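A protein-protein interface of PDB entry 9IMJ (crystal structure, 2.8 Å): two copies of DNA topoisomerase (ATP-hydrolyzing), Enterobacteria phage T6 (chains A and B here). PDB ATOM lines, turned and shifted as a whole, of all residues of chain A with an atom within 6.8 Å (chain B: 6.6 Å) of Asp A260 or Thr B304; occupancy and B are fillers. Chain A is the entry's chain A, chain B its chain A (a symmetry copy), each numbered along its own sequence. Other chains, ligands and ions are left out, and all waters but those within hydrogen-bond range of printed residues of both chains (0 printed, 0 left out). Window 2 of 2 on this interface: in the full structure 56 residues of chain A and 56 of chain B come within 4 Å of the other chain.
OG1 of Thr B304 is in hydrogen-bond range of OD1 of Asp A260 (3.2 Å).
The side-chain carboxylate of Glu A32 is in salt-bridge range of the side-chain amino group of Lys B305 (3.9 Å).
N of Ala B306 sits close to OD1 of Asp A260 (3.3 Å).
The side-chain carboxylate (OE1) of Glu A32 lies within hydrogen-bond range of the indole nitrogen (NE1) of Trp A39, at 2.8 Å.
The backbone carbonyl oxygen of Glu A310 lies close to the backbone NH of Gly A261 (3.5 Å).
N of Asp A260 is in hydrogen-bond range of OG of Ser A258.
The backbone NH (N) of Arg B307 is in hydrogen-bond range of the side-chain hydroxyl (OG1) of Thr B304.
The backbone NH (N) of Phe A262 is in hydrogen-bond range of the side-chain carboxylate (OE2) of Glu A310 (3.2 Å).
OG1 of Thr B304 lies close to N of Ala B306.
Among the printed residues, pairs that only touch across the chains: Gly A261 with Ala B306 and Glu A310 with Ala B306.
Of chain B, only Thr B304 and Ala B306 come within 4 Å of Asp A260.
Printed residues of chain B within 4 Å of Gly A261: Ala B306.
Thr B304 touches just one residue of chain A: Asp A260 (3.2 Å).
Of the printed residues of chain A, Ala B306 touches Asp A260, Gly A261 and Glu A310.
Arg B307 touches none of the printed residues of chain A.
Val B308 touches none of the printed residues of chain A.
Of the 10 printed residues of chain A, 4 touch a printed residue of chain B.
Along chain B the printed residues that touch a printed residue of chain A span positions 304 to 306.
Among the printed residues, 5 pairs touch across the chains.
Among the printed residues, Asp or Glu carboxylates within 4 Å of a Lys or Arg side-chain nitrogen of the other chain: Glu A32 with Lys B305 (3.9 Å).
No position is printed for both chains.
Of the 5 pairs that touch across the chains among the printed residues, none has its exchanged pair printed and touching as well.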
ATOM      1  N   GLU A  32      16.151 -33.468  28.957  1.00  0.00           N
ATOM      2  CA  GLU A  32      15.313 -32.441  29.555  1.00  0.00           C
ATOM      3  C   GLU A  32      13.869 -32.792  29.270  1.00  0.00           C
ATOM      4  O   GLU A  32      13.548 -33.268  28.183  1.00  0.00           O
ATOM      5  CB  GLU A  32      15.638 -31.057  29.001  1.00  0.00           C
ATOM      6  CG  GLU A  32      17.114 -30.789  28.853  1.00  0.00           C
ATOM      7  CD  GLU A  32      17.521 -29.370  29.219  1.00  0.00           C
ATOM      8  OE1 GLU A  32      16.765 -28.415  28.896  1.00  0.00           O
ATOM      9  OE2 GLU A  32      18.624 -29.222  29.800  1.00  0.00           O
ATOM     10  N   TRP A  39      10.450 -28.337  34.581  1.00  0.00           N
ATOM     11  CA  TRP A  39      11.370 -28.687  33.514  1.00  0.00           C
ATOM     12  C   TRP A  39      12.719 -29.052  34.135  1.00  0.00           C
ATOM     13  O   TRP A  39      13.643 -28.233  34.167  1.00  0.00           O
ATOM     14  CB  TRP A  39      11.487 -27.521  32.520  1.00  0.00           C
ATOM     15  CG  TRP A  39      12.371 -27.828  31.359  1.00  0.00           C
ATOM     16  CD1 TRP A  39      13.720 -27.615  31.253  1.00  0.00           C
ATOM     17  CD2 TRP A  39      11.965 -28.449  30.142  1.00  0.00           C
ATOM     18  NE1 TRP A  39      14.177 -28.052  30.027  1.00  0.00           N
ATOM     19  CE2 TRP A  39      13.115 -28.567  29.327  1.00  0.00           C
ATOM     20  CE3 TRP A  39      10.736 -28.907  29.657  1.00  0.00           C
ATOM     21  CZ2 TRP A  39      13.069 -29.121  28.062  1.00  0.00           C
ATOM     22  CZ3 TRP A  39      10.690 -29.452  28.408  1.00  0.00           C
ATOM     23  CH2 TRP A  39      11.851 -29.562  27.620  1.00  0.00           C
ATOM     24  N   SER A 258       7.843 -19.527  30.313  1.00  0.00           N
ATOM     25  CA  SER A 258       9.030 -20.360  30.283  1.00  0.00           C
ATOM     26  C   SER A 258      10.244 -19.451  30.382  1.00  0.00           C
ATOM     27  O   SER A 258      10.250 -18.353  29.816  1.00  0.00           O
ATOM     28  CB  SER A 258       9.162 -21.225  29.029  1.00  0.00           C
ATOM     29  OG  SER A 258      10.482 -21.743  28.970  1.00  0.00           O
ATOM     30  N   PRO A 259      11.254 -19.869  31.105  1.00  0.00           N
ATOM     31  CA  PRO A 259      12.494 -19.096  31.168  1.00  0.00           C
ATOM     32  C   PRO A 259      13.452 -19.390  30.017  1.00  0.00           C
ATOM     33  O   PRO A 259      14.313 -18.559  29.725  1.00  0.00           O
ATOM     34  CB  PRO A 259      13.106 -19.542  32.502  1.00  0.00           C
ATOM     35  CG  PRO A 259      12.595 -20.921  32.709  1.00  0.00           C
ATOM     36  CD  PRO A 259      11.237 -20.984  32.069  1.00  0.00           C
ATOM     37  N   ASP A 260      13.361 -20.573  29.372  1.00  0.00           N
ATOM     38  CA  ASP A 260      14.404 -21.050  28.443  1.00  0.00           C
ATOM     39  C   ASP A 260      13.796 -21.871  27.293  1.00  0.00           C
ATOM     40  O   ASP A 260      13.944 -23.104  27.239  1.00  0.00           O
ATOM     41  CB  ASP A 260      15.457 -21.878  29.179  1.00  0.00           C
ATOM     42  CG  ASP A 260      16.853 -21.659  28.642  1.00  0.00           C
ATOM     43  OD1 ASP A 260      17.016 -20.970  27.618  1.00  0.00           O
ATOM     44  OD2 ASP A 260      17.795 -22.219  29.233  1.00  0.00           O
ATOM     45  N   GLY A 261      13.124 -21.170  26.371  1.00  0.00           N
ATOM     46  CA  GLY A 261      12.606 -21.738  25.141  1.00  0.00           C
ATOM     47  C   GLY A 261      11.234 -22.391  25.280  1.00  0.00           C
ATOM     48  O   GLY A 261      10.803 -22.791  26.362  1.00  0.00           O
ATOM     49  N   PHE A 262      10.536 -22.490  24.150  1.00  0.00           N
ATOM     50  CA  PHE A 262       9.268 -23.198  24.112  1.00  0.00           C
ATOM     51  C   PHE A 262       9.405 -24.548  24.785  1.00  0.00           C
ATOM     52  O   PHE A 262      10.279 -25.352  24.429  1.00  0.00           O
ATOM     53  CB  PHE A 262       8.818 -23.378  22.672  1.00  0.00           C
ATOM     54  CG  PHE A 262       7.383 -23.807  22.516  1.00  0.00           C
ATOM     55  CD1 PHE A 262       6.340 -22.987  22.930  1.00  0.00           C
ATOM     56  CD2 PHE A 262       7.080 -25.011  21.905  1.00  0.00           C
ATOM     57  CE1 PHE A 262       5.014 -23.373  22.748  1.00  0.00           C
ATOM     58  CE2 PHE A 262       5.762 -25.400  21.708  1.00  0.00           C
ATOM     59  CZ  PHE A 262       4.728 -24.584  22.131  1.00  0.00           C
ATOM     60  N   ARG A 263       8.570 -24.764  25.796  1.00  0.00           N
ATOM     61  CA  ARG A 263       8.376 -26.069  26.394  1.00  0.00           C
ATOM     62  C   ARG A 263       6.911 -26.445  26.230  1.00  0.00           C
ATOM     63  O   ARG A 263       6.033 -25.574  26.162  1.00  0.00           O
ATOM     64  CB  ARG A 263       8.787 -26.083  27.884  1.00  0.00           C
ATOM     65  CG  ARG A 263      10.263 -25.901  28.133  1.00  0.00           C
ATOM     66  CD  ARG A 263      10.497 -25.502  29.559  1.00  0.00           C
ATOM     67  NE  ARG A 263      11.883 -25.131  29.801  1.00  0.00           N
ATOM     68  CZ  ARG A 263      12.301 -24.532  30.907  1.00  0.00           C
ATOM     69  NH1 ARG A 263      11.470 -24.285  31.909  1.00  0.00           N
ATOM     70  NH2 ARG A 263      13.580 -24.164  31.004  1.00  0.00           N
ATOM     71  N   GLU A 310       8.850 -18.934  22.128  1.00  0.00           N
ATOM     72  CA  GLU A 310      10.014 -19.248  22.960  1.00  0.00           C
ATOM     73  C   GLU A 310       9.862 -18.762  24.404  1.00  0.00           C
ATOM     74  O   GLU A 310      10.807 -18.893  25.188  1.00  0.00           O
ATOM     75  CB  GLU A 310      11.297 -18.670  22.345  1.00  0.00           C
ATOM     76  CG  GLU A 310      11.875 -19.556  21.231  1.00  0.00           C
ATOM     77  CD  GLU A 310      12.526 -20.871  21.729  1.00  0.00           C
ATOM     78  OE1 GLU A 310      13.558 -20.776  22.439  1.00  0.00           O
ATOM     79  OE2 GLU A 310      12.038 -21.990  21.381  1.00  0.00           O
ATOM     80  N   CYS A 311       8.708 -18.195  24.761  1.00  0.00           N
ATOM     81  CA  CYS A 311       8.451 -17.739  26.113  1.00  0.00           C
ATOM     82  C   CYS A 311       7.307 -18.478  26.795  1.00  0.00           C
ATOM     83  O   CYS A 311       7.081 -18.257  27.993  1.00  0.00           O
ATOM     84  CB  CYS A 311       8.125 -16.239  26.125  1.00  0.00           C
ATOM     85  SG  CYS A 311       9.314 -15.060  25.402  1.00  0.00           S
ATOM     86  N   CYS B 288      27.599 -23.450  22.971  1.00  0.00           N
ATOM     87  CA  CYS B 288      27.078 -22.460  23.901  1.00  0.00           C
ATOM     88  C   CYS B 288      27.911 -22.351  25.184  1.00  0.00           C
ATOM     89  O   CYS B 288      27.950 -21.270  25.787  1.00  0.00           O
ATOM     90  CB  CYS B 288      25.619 -22.802  24.233  1.00  0.00           C
ATOM     91  SG  CYS B 288      24.324 -22.248  23.050  1.00  0.00           S
ATOM     92  N   ILE B 292      28.784 -18.516  26.015  1.00  0.00           N
ATOM     93  CA  ILE B 292      28.189 -17.746  27.118  1.00  0.00           C
ATOM     94  C   ILE B 292      29.228 -17.336  28.154  1.00  0.00           C
ATOM     95  O   ILE B 292      29.141 -16.206  28.661  1.00  0.00           O
ATOM     96  CB  ILE B 292      26.988 -18.496  27.711  1.00  0.00           C
ATOM     97  CG1 ILE B 292      26.134 -19.112  26.602  1.00  0.00           C
ATOM     98  CG2 ILE B 292      26.119 -17.542  28.531  1.00  0.00           C
ATOM     99  CD1 ILE B 292      24.730 -19.513  27.033  1.00  0.00           C
ATOM    100  N   ASP B 302      23.966 -11.498  30.441  1.00  0.00           N
ATOM    101  CA  ASP B 302      23.412 -12.834  30.547  1.00  0.00           C
ATOM    102  C   ASP B 302      22.426 -13.017  29.405  1.00  0.00           C
ATOM    103  O   ASP B 302      21.432 -12.285  29.307  1.00  0.00           O
ATOM    104  CB  ASP B 302      22.784 -13.044  31.920  1.00  0.00           C
ATOM    105  CG  ASP B 302      23.815 -12.974  33.016  1.00  0.00           C
ATOM    106  OD1 ASP B 302      25.018 -13.039  32.661  1.00  0.00           O
ATOM    107  OD2 ASP B 302      23.445 -12.863  34.207  1.00  0.00           O
ATOM    108  N   VAL B 303      22.755 -13.950  28.510  1.00  0.00           N
ATOM    109  CA  VAL B 303      21.852 -14.457  27.484  1.00  0.00           C
ATOM    110  C   VAL B 303      21.747 -15.968  27.685  1.00  0.00           C
ATOM    111  O   VAL B 303      22.704 -16.623  28.123  1.00  0.00           O
ATOM    112  CB  VAL B 303      22.317 -14.118  26.034  1.00  0.00           C
ATOM    113  CG1 VAL B 303      22.004 -12.658  25.661  1.00  0.00           C
ATOM    114  CG2 VAL B 303      23.806 -14.440  25.831  1.00  0.00           C
ATOM    115  N   THR B 304      20.576 -16.518  27.350  1.00  0.00           N
ATOM    116  CA  THR B 304      20.285 -17.931  27.550  1.00  0.00           C
ATOM    117  C   THR B 304      20.787 -18.782  26.384  1.00  0.00           C
ATOM    118  O   THR B 304      21.016 -18.298  25.270  1.00  0.00           O
ATOM    119  CB  THR B 304      18.785 -18.160  27.717  1.00  0.00           C
ATOM    120  OG1 THR B 304      18.170 -18.196  26.421  1.00  0.00           O
ATOM    121  CG2 THR B 304      18.157 -17.043  28.536  1.00  0.00           C
ATOM    122  N   LYS B 305      20.931 -20.082  26.655  1.00  0.00           N
ATOM    123  CA  LYS B 305      21.313 -21.026  25.611  1.00  0.00           C
ATOM    124  C   LYS B 305      20.228 -21.144  24.548  1.00  0.00           C
ATOM    125  O   LYS B 305      20.525 -21.430  23.386  1.00  0.00           O
ATOM    126  CB  LYS B 305      21.633 -22.379  26.252  1.00  0.00           C
ATOM    127  CG  LYS B 305      21.333 -23.625  25.430  1.00  0.00           C
ATOM    128  CD  LYS B 305      21.652 -24.905  26.232  1.00  0.00           C
ATOM    129  CE  LYS B 305      20.381 -25.539  26.839  1.00  0.00           C
ATOM    130  NZ  LYS B 305      20.603 -26.227  28.169  1.00  0.00           N
ATOM    131  N   ALA B 306      18.970 -20.909  24.915  1.00  0.00           N
ATOM    132  CA  ALA B 306      17.922 -20.852  23.903  1.00  0.00           C
ATOM    133  C   ALA B 306      18.017 -19.583  23.087  1.00  0.00           C
ATOM    134  O   ALA B 306      17.646 -19.578  21.912  1.00  0.00           O
ATOM    135  CB  ALA B 306      16.543 -20.934  24.544  1.00  0.00           C
ATOM    136  N   ARG B 307      18.500 -18.500  23.703  1.00  0.00           N
ATOM    137  CA  ARG B 307      18.669 -17.231  22.996  1.00  0.00           C
ATOM    138  C   ARG B 307      19.737 -17.329  21.911  1.00  0.00           C
ATOM    139  O   ARG B 307      19.512 -16.899  20.775  1.00  0.00           O
ATOM    140  CB  ARG B 307      19.038 -16.124  23.984  1.00  0.00           C
ATOM    141  CG  ARG B 307      19.274 -14.795  23.295  1.00  0.00           C
ATOM    142  CD  ARG B 307      18.020 -14.000  23.329  1.00  0.00           C
ATOM    143  NE  ARG B 307      17.224 -14.227  22.135  1.00  0.00           N
ATOM    144  CZ  ARG B 307      16.276 -13.402  21.717  1.00  0.00           C
ATOM    145  NH1 ARG B 307      16.041 -12.256  22.340  1.00  0.00           N
ATOM    146  NH2 ARG B 307      15.553 -13.733  20.653  1.00  0.00           N
ATOM    147  N   VAL B 308      20.926 -17.829  22.276  1.00  0.00           N
ATOM    148  CA  VAL B 308      21.985 -18.112  21.308  1.00  0.00           C
ATOM    149  C   VAL B 308      21.434 -18.913  20.138  1.00  0.00           C
ATOM    150  O   VAL B 308      21.522 -18.504  18.974  1.00  0.00           O
ATOM    151  CB  VAL B 308      23.137 -18.877  21.978  1.00  0.00           C
ATOM    152  CG1 VAL B 308      24.111 -19.348  20.930  1.00  0.00           C
ATOM    153  CG2 VAL B 308      23.799 -18.025  23.044  1.00  0.00           C
ATOM    154  N   LYS B 309      20.847 -20.063  20.435  1.00  0.00           N
ATOM    155  CA  LYS B 309      20.467 -20.964  19.366  1.00  0.00           C
ATOM    156  C   LYS B 309      19.211 -20.494  18.649  1.00  0.00           C
ATOM    157  O   LYS B 309      19.039 -20.774  17.464  1.00  0.00           O
ATOM    158  CB  LYS B 309      20.339 -22.385  19.927  1.00  0.00           C
ATOM    159  CG  LYS B 309      18.941 -22.857  20.229  1.00  0.00           C
ATOM    160  CD  LYS B 309      19.002 -24.130  21.086  1.00  0.00           C
ATOM    161  CE  LYS B 309      19.556 -25.316  20.294  1.00  0.00           C
ATOM    162  NZ  LYS B 309      18.788 -26.586  20.509  1.00  0.00           N
ATOM    163  N   ILE B 366      22.246 -12.089  19.119  1.00  0.00           N
ATOM    164  CA  ILE B 366      22.312 -12.759  20.424  1.00  0.00           C
ATOM    165  C   ILE B 366      22.250 -11.737  21.548  1.00  0.00           C
ATOM    166  O   ILE B 366      21.290 -11.672  22.328  1.00  0.00           O
ATOM    167  CB  ILE B 366      23.603 -13.590  20.547  1.00  0.00           C
ATOM    168  CG1 ILE B 366      23.755 -14.605  19.424  1.00  0.00           C
ATOM    169  CG2 ILE B 366      23.610 -14.318  21.874  1.00  0.00           C
ATOM    170  CD1 ILE B 366      22.534 -15.323  19.126  1.00  0.00           C
